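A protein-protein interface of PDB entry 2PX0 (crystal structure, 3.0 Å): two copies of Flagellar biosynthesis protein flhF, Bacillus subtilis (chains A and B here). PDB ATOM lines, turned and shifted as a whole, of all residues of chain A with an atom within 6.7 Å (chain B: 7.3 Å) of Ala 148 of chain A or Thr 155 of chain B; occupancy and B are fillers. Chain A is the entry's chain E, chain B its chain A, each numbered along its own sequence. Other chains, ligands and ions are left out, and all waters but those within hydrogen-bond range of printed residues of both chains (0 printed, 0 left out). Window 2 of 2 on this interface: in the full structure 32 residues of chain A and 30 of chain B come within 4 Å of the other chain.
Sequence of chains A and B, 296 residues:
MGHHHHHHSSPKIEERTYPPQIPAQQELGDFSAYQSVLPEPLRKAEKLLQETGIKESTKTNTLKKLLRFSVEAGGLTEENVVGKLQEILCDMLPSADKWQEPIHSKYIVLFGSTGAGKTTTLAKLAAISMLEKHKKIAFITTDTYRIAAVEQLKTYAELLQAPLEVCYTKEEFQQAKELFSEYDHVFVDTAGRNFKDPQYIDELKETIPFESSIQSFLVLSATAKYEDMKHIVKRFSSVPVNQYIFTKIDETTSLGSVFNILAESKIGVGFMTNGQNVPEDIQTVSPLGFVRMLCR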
ATOM      1  N   THR A 144     -13.858  30.720  27.383  1.00  0.00           N
ATOM      2  CA  THR A 144     -13.335  29.905  28.466  1.00  0.00           C
ATOM      3  C   THR A 144     -14.210  28.681  28.646  1.00  0.00           C
ATOM      4  O   THR A 144     -13.801  27.562  28.358  1.00  0.00           O
ATOM      5  CB  THR A 144     -13.336  30.684  29.794  1.00  0.00           C
ATOM      6  OG1 THR A 144     -12.317  31.697  29.766  1.00  0.00           O
ATOM      7  CG2 THR A 144     -13.113  29.734  30.972  1.00  0.00           C
ATOM      8  N   ARG A 146     -15.975  26.494  27.435  1.00  0.00           N
ATOM      9  CA  ARG A 146     -15.854  25.195  26.770  1.00  0.00           C
ATOM     10  C   ARG A 146     -14.476  24.532  26.823  1.00  0.00           C
ATOM     11  O   ARG A 146     -13.442  25.182  26.652  1.00  0.00           O
ATOM     12  CB  ARG A 146     -16.294  25.303  25.309  1.00  0.00           C
ATOM     13  CG  ARG A 146     -16.642  23.963  24.658  1.00  0.00           C
ATOM     14  CD  ARG A 146     -16.025  23.854  23.276  1.00  0.00           C
ATOM     15  NE  ARG A 146     -16.448  24.928  22.381  1.00  0.00           N
ATOM     16  CZ  ARG A 146     -15.776  25.304  21.296  1.00  0.00           C
ATOM     17  NH1 ARG A 146     -14.639  24.703  20.960  1.00  0.00           N
ATOM     18  NH2 ARG A 146     -16.244  26.284  20.541  1.00  0.00           N
ATOM     19  N   ILE A 147     -14.493  23.222  27.048  1.00  0.00           N
ATOM     20  CA  ILE A 147     -13.296  22.389  27.127  1.00  0.00           C
ATOM     21  C   ILE A 147     -12.428  22.489  25.877  1.00  0.00           C
ATOM     22  O   ILE A 147     -12.899  22.264  24.753  1.00  0.00           O
ATOM     23  CB  ILE A 147     -13.691  20.914  27.314  1.00  0.00           C
ATOM     24  CG1 ILE A 147     -14.869  20.584  26.359  1.00  0.00           C
ATOM     25  CG2 ILE A 147     -14.010  20.649  28.783  1.00  0.00           C
ATOM     26  CD1 ILE A 147     -15.485  19.170  26.457  1.00  0.00           C
ATOM     27  N   ALA A 148     -11.157  22.823  26.087  1.00  0.00           N
ATOM     28  CA  ALA A 148     -10.177  22.948  25.005  1.00  0.00           C
ATOM     29  C   ALA A 148     -10.623  23.863  23.870  1.00  0.00           C
ATOM     30  O   ALA A 148     -10.042  23.842  22.780  1.00  0.00           O
ATOM     31  CB  ALA A 148      -9.848  21.575  24.454  1.00  0.00           C
ATOM     32  N   ALA A 149     -11.644  24.671  24.137  1.00  0.00           N
ATOM     33  CA  ALA A 149     -12.179  25.592  23.139  1.00  0.00           C
ATOM     34  C   ALA A 149     -11.124  26.540  22.562  1.00  0.00           C
ATOM     35  O   ALA A 149     -11.193  26.929  21.391  1.00  0.00           O
ATOM     36  CB  ALA A 149     -13.317  26.399  23.747  1.00  0.00           C
ATOM     37  N   VAL A 150     -10.148  26.896  23.391  1.00  0.00           N
ATOM     38  CA  VAL A 150      -9.088  27.817  23.003  1.00  0.00           C
ATOM     39  C   VAL A 150      -8.059  27.235  22.052  1.00  0.00           C
ATOM     40  O   VAL A 150      -7.574  27.933  21.162  1.00  0.00           O
ATOM     41  CB  VAL A 150      -8.353  28.354  24.243  1.00  0.00           C
ATOM     42  CG1 VAL A 150      -7.234  29.271  23.829  1.00  0.00           C
ATOM     43  CG2 VAL A 150      -9.324  29.094  25.131  1.00  0.00           C
ATOM     44  N   GLU A 151      -7.723  25.963  22.235  1.00  0.00           N
ATOM     45  CA  GLU A 151      -6.729  25.328  21.376  1.00  0.00           C
ATOM     46  C   GLU A 151      -6.930  25.672  19.907  1.00  0.00           C
ATOM     47  O   GLU A 151      -5.964  25.795  19.154  1.00  0.00           O
ATOM     48  CB  GLU A 151      -6.754  23.809  21.556  1.00  0.00           C
ATOM     49  CG  GLU A 151      -5.774  23.315  22.596  1.00  0.00           C
ATOM     50  CD  GLU A 151      -4.348  23.726  22.279  1.00  0.00           C
ATOM     51  OE1 GLU A 151      -3.814  23.283  21.235  1.00  0.00           O
ATOM     52  OE2 GLU A 151      -3.766  24.494  23.075  1.00  0.00           O
ATOM     53  N   GLN A 152      -8.187  25.839  19.513  1.00  0.00           N
ATOM     54  CA  GLN A 152      -8.531  26.155  18.134  1.00  0.00           C
ATOM     55  C   GLN A 152      -7.837  27.418  17.645  1.00  0.00           C
ATOM     56  O   GLN A 152      -6.991  27.362  16.758  1.00  0.00           O
ATOM     57  CB  GLN A 152     -10.043  26.330  18.000  1.00  0.00           C
ATOM     58  CG  GLN A 152     -10.593  26.028  16.614  1.00  0.00           C
ATOM     59  CD  GLN A 152     -12.053  26.419  16.476  1.00  0.00           C
ATOM     60  OE1 GLN A 152     -12.869  26.138  17.358  1.00  0.00           O
ATOM     61  NE2 GLN A 152     -12.391  27.060  15.366  1.00  0.00           N
ATOM     62  N   ALA B 148      -7.903  21.975  14.834  1.00  0.00           N
ATOM     63  CA  ALA B 148      -7.844  21.761  16.282  1.00  0.00           C
ATOM     64  C   ALA B 148      -8.941  20.818  16.782  1.00  0.00           C
ATOM     65  O   ALA B 148      -9.009  20.516  17.983  1.00  0.00           O
ATOM     66  CB  ALA B 148      -7.916  23.108  17.029  1.00  0.00           C
ATOM     67  N   ALA B 149      -9.789  20.353  15.865  1.00  0.00           N
ATOM     68  CA  ALA B 149     -10.876  19.453  16.224  1.00  0.00           C
ATOM     69  C   ALA B 149     -10.367  18.254  17.032  1.00  0.00           C
ATOM     70  O   ALA B 149     -10.966  17.852  18.032  1.00  0.00           O
ATOM     71  CB  ALA B 149     -11.573  18.973  14.973  1.00  0.00           C
ATOM     72  N   VAL B 150      -9.259  17.681  16.584  1.00  0.00           N
ATOM     73  CA  VAL B 150      -8.671  16.536  17.253  1.00  0.00           C
ATOM     74  C   VAL B 150      -8.173  16.897  18.645  1.00  0.00           C
ATOM     75  O   VAL B 150      -8.698  16.397  19.645  1.00  0.00           O
ATOM     76  CB  VAL B 150      -7.507  15.959  16.421  1.00  0.00           C
ATOM     77  CG1 VAL B 150      -6.713  14.958  17.245  1.00  0.00           C
ATOM     78  CG2 VAL B 150      -8.064  15.274  15.173  1.00  0.00           C
ATOM     79  N   GLU B 151      -7.157  17.758  18.703  1.00  0.00           N
ATOM     80  CA  GLU B 151      -6.574  18.195  19.973  1.00  0.00           C
ATOM     81  C   GLU B 151      -7.593  18.330  21.117  1.00  0.00           C
ATOM     82  O   GLU B 151      -7.293  17.982  22.263  1.00  0.00           O
ATOM     83  CB  GLU B 151      -5.855  19.530  19.776  1.00  0.00           C
ATOM     84  CG  GLU B 151      -4.558  19.429  18.997  1.00  0.00           C
ATOM     85  CD  GLU B 151      -4.047  20.787  18.540  1.00  0.00           C
ATOM     86  OE1 GLU B 151      -4.550  21.297  17.514  1.00  0.00           O
ATOM     87  OE2 GLU B 151      -3.149  21.349  19.211  1.00  0.00           O
ATOM     88  N   GLN B 152      -8.792  18.823  20.798  1.00  0.00           N
ATOM     89  CA  GLN B 152      -9.846  19.025  21.795  1.00  0.00           C
ATOM     90  C   GLN B 152     -10.543  17.747  22.244  1.00  0.00           C
ATOM     91  O   GLN B 152     -10.710  17.520  23.441  1.00  0.00           O
ATOM     92  CB  GLN B 152     -10.877  20.017  21.262  1.00  0.00           C
ATOM     93  CG  GLN B 152     -10.329  21.430  21.126  1.00  0.00           C
ATOM     94  CD  GLN B 152     -11.287  22.373  20.427  1.00  0.00           C
ATOM     95  OE1 GLN B 152     -11.299  22.475  19.195  1.00  0.00           O
ATOM     96  NE2 GLN B 152     -12.110  23.059  21.209  1.00  0.00           N
ATOM     97  N   LEU B 153     -10.956  16.915  21.286  1.00  0.00           N
ATOM     98  CA  LEU B 153     -11.624  15.650  21.605  1.00  0.00           C
ATOM     99  C   LEU B 153     -10.635  14.723  22.295  1.00  0.00           C
ATOM    100  O   LEU B 153     -11.022  13.853  23.069  1.00  0.00           O
ATOM    101  CB  LEU B 153     -12.160  14.977  20.339  1.00  0.00           C
ATOM    102  CG  LEU B 153     -12.837  13.610  20.505  1.00  0.00           C
ATOM    103  CD1 LEU B 153     -13.985  13.687  21.508  1.00  0.00           C
ATOM    104  CD2 LEU B 153     -13.357  13.148  19.162  1.00  0.00           C
ATOM    105  N   LYS B 154      -9.352  14.912  22.009  1.00  0.00           N
ATOM    106  CA  LYS B 154      -8.326  14.095  22.638  1.00  0.00           C
ATOM    107  C   LYS B 154      -8.178  14.539  24.085  1.00  0.00           C
ATOM    108  O   LYS B 154      -8.355  13.744  25.010  1.00  0.00           O
ATOM    109  CB  LYS B 154      -6.979  14.245  21.917  1.00  0.00           C
ATOM    110  CG  LYS B 154      -5.855  13.429  22.559  1.00  0.00           C
ATOM    111  CD  LYS B 154      -6.248  11.948  22.683  1.00  0.00           C
ATOM    112  CE  LYS B 154      -5.160  11.099  23.350  1.00  0.00           C
ATOM    113  NZ  LYS B 154      -5.535   9.653  23.444  1.00  0.00           N
ATOM    114  N   THR B 155      -7.864  15.817  24.277  1.00  0.00           N
ATOM    115  CA  THR B 155      -7.696  16.345  25.620  1.00  0.00           C
ATOM    116  C   THR B 155      -8.996  16.271  26.411  1.00  0.00           C
ATOM    117  O   THR B 155      -9.071  16.755  27.541  1.00  0.00           O
ATOM    118  CB  THR B 155      -7.189  17.797  25.600  1.00  0.00           C
ATOM    119  OG1 THR B 155      -8.157  18.641  24.972  1.00  0.00           O
ATOM    120  CG2 THR B 155      -5.862  17.876  24.842  1.00  0.00           C
ATOM    121  N   TYR B 156     -10.022  15.680  25.805  1.00  0.00           N
ATOM    122  CA  TYR B 156     -11.298  15.503  26.486  1.00  0.00           C
ATOM    123  C   TYR B 156     -11.430  14.032  26.821  1.00  0.00           C
ATOM    124  O   TYR B 156     -11.811  13.670  27.935  1.00  0.00           O
ATOM    125  CB  TYR B 156     -12.469  15.880  25.603  1.00  0.00           C
ATOM    126  CG  TYR B 156     -13.785  15.440  26.206  1.00  0.00           C
ATOM    127  CD1 TYR B 156     -14.284  16.054  27.353  1.00  0.00           C
ATOM    128  CD2 TYR B 156     -14.491  14.362  25.678  1.00  0.00           C
ATOM    129  CE1 TYR B 156     -15.447  15.605  27.966  1.00  0.00           C
ATOM    130  CE2 TYR B 156     -15.659  13.900  26.282  1.00  0.00           C
ATOM    131  CZ  TYR B 156     -16.132  14.524  27.431  1.00  0.00           C
ATOM    132  OH  TYR B 156     -17.269  14.054  28.065  1.00  0.00           O
ATOM    133  N   ALA B 157     -11.127  13.191  25.831  1.00  0.00           N
ATOM    134  CA  ALA B 157     -11.187  11.747  26.008  1.00  0.00           C
ATOM    135  C   ALA B 157     -10.214  11.394  27.117  1.00  0.00           C
ATOM    136  O   ALA B 157     -10.412  10.419  27.835  1.00  0.00           O
ATOM    137  CB  ALA B 157     -10.805  11.034  24.725  1.00  0.00           C
ATOM    138  N   GLU B 158      -9.162  12.199  27.259  1.00  0.00           N
ATOM    139  CA  GLU B 158      -8.178  11.961  28.309  1.00  0.00           C
ATOM    140  C   GLU B 158      -8.880  12.125  29.654  1.00  0.00           C
ATOM    141  O   GLU B 158      -8.659  11.335  30.574  1.00  0.00           O
ATOM    142  CB  GLU B 158      -7.009  12.951  28.215  1.00  0.00           C
ATOM    143  CG  GLU B 158      -6.188  12.854  26.927  1.00  0.00           C
ATOM    144  CD  GLU B 158      -5.064  13.892  26.859  1.00  0.00           C
ATOM    145  OE1 GLU B 158      -5.185  14.958  27.512  1.00  0.00           O
ATOM    146  OE2 GLU B 158      -4.068  13.652  26.135  1.00  0.00           O
ATOM    147  N   LEU B 159      -9.725  13.151  29.764  1.00  0.00           N
ATOM    148  CA  LEU B 159     -10.464  13.400  31.003  1.00  0.00           C
ATOM    149  C   LEU B 159     -11.318  12.189  31.342  1.00  0.00           C
ATOM    150  O   LEU B 159     -11.221  11.628  32.428  1.00  0.00           O
ATOM    151  CB  LEU B 159     -11.380  14.625  30.865  1.00  0.00           C
ATOM    152  CG  LEU B 159     -10.837  16.046  31.044  1.00  0.00           C
ATOM    153  CD1 LEU B 159     -11.982  17.041  30.942  1.00  0.00           C
ATOM    154  CD2 LEU B 159     -10.174  16.183  32.395  1.00  0.00           C
ATOM    155  N   LEU B 160     -12.160  11.792  30.398  1.00  0.00           N
ATOM    156  CA  LEU B 160     -13.035  10.651  30.593  1.00  0.00           C
ATOM    157  C   LEU B 160     -12.146   9.423  30.704  1.00  0.00           C
ATOM    158  O   LEU B 160     -12.614   8.319  30.971  1.00  0.00           O
ATOM    159  CB  LEU B 160     -13.979  10.525  29.396  1.00  0.00           C
ATOM    160  CG  LEU B 160     -15.362   9.934  29.648  1.00  0.00           C
ATOM    161  CD1 LEU B 160     -16.046  10.724  30.744  1.00  0.00           C
ATOM    162  CD2 LEU B 160     -16.179   9.975  28.359  1.00  0.00           C
ATOM    163  N   LEU B 164      -8.720   6.992  22.020  1.00  0.00           N
ATOM    164  CA  LEU B 164      -9.179   7.687  20.825  1.00  0.00           C
ATOM    165  C   LEU B 164      -8.223   7.407  19.668  1.00  0.00           C
ATOM    166  O   LEU B 164      -7.004   7.349  19.861  1.00  0.00           O
ATOM    167  CB  LEU B 164      -9.250   9.190  21.094  1.00  0.00           C
ATOM    168  CG  LEU B 164      -9.742  10.100  19.966  1.00  0.00           C
ATOM    169  CD1 LEU B 164     -10.029  11.467  20.543  1.00  0.00           C
ATOM    170  CD2 LEU B 164      -8.710  10.205  18.856  1.00  0.00           C
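Ala 148 of chain A touches just these residues of chain B: Gln 152 and Thr 155. Printed residues of chain A within 4 Å of Thr 155 of chain B: Ala 148 (3.4 Å). Printed residues of chain B within 4 Å of Ile 147 of chain A: Gln 152 and Tyr 156. Of the printed residues of chain A, Ala 148 of chain B touches Glu 151 and Gln 152. Of the printed residues of chain B, Arg 146 of chain A touches Gln 152 (3.0 Å). Of the printed residues of chain A, Glu 151 of chain B touches Glu 151. Printed residues of chain B within 4 Å of Ala 149 of chain A: Gln 152. Glu 158 of chain B touches none of the printed residues of chain A. Leu 159 of chain B touches none of the printed residues of chain A. The nearest residue of chain B that does not touch Ala 148 of chain A is Glu 151 of chain B (4.9 Å). The nearest residue of chain A that does not touch Thr 155 of chain B is Glu 151 of chain A (5.8 Å).
Ala 148 of chain A touches Gln 152 of chain B, and with the chains exchanged Gln 152 of chain A touches Ala 148 of chain B. Ala 149 of chain A touches Gln 152 of chain B, but with the chains exchanged Gln 152 of chain A does not touch Ala 149 of chain B (5.8 Å). Glu 151 of chain A touches Ala 148 of chain B, but with the chains exchanged Ala 148 of chain A does not touch Glu 151 of chain B (4.9 Å). Glu 151 of chain B touches its own counterpart, Glu 151 of chain A.
The side-chain amide nitrogen (NE2) of Gln 152 of chain B sits close to the guanidinium group (NH1) of Arg 146 of chain A. The side-chain amide nitrogen of Gln 152 of chain B lies within hydrogen-bond range of the backbone carbonyl oxygen of Ala 148 of chain A (2.7 Å). The side-chain amide nitrogen of Gln 152 of chain B lies close to the backbone NH of Ala 149 of chain A, 3.4 Å away. The side-chain carboxylate (OE2) of Glu 151 of chain B sits close to the side-chain carboxylate (OE1) of Glu 151 of chain A (2.9 Å).
O of Ala 148 of chain B lies close to OE1 of Gln 152 of chain B (3.2 Å). O of Glu 151 of chain B is in hydrogen-bond range of OG1 of Thr 155 of chain B. The backbone carbonyl oxygen of Gln 152 of chain B sits at hydrogen-bond distance from the side-chain hydroxyl of Thr 155 of chain B.
Gln 152 of chain B touches Ile 147 of chain A. Ile 147 of chain A touches Tyr 156 of chain B. Ala 148 of chain A touches Thr 155 of chain B (CB to OG1, 3.4 Å). Ala 148 of chain B touches Glu 151 of chain A (CB to O, 3.9 Å). Ala 148 of chain B touches Gln 152 of chain A (CB to CA, 3.3 Å).
Printed residues of chain B that touch a printed residue of chain A: Ala 148, Glu 151, Gln 152, Thr 155 and Tyr 156. Along chain B the printed residues that touch a printed residue of chain A span positions 148 to 156. Printed residues of chain A that touch a printed residue of chain B: Arg 146, Ile 147, Ala 148, Ala 149, Glu 151 and Gln 152. Among the printed residues, 9 pairs touch across the chains. Among the printed residues, no Asp or Glu carboxylate lies within 4 Å of a Lys or Arg side-chain nitrogen of the other chain.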
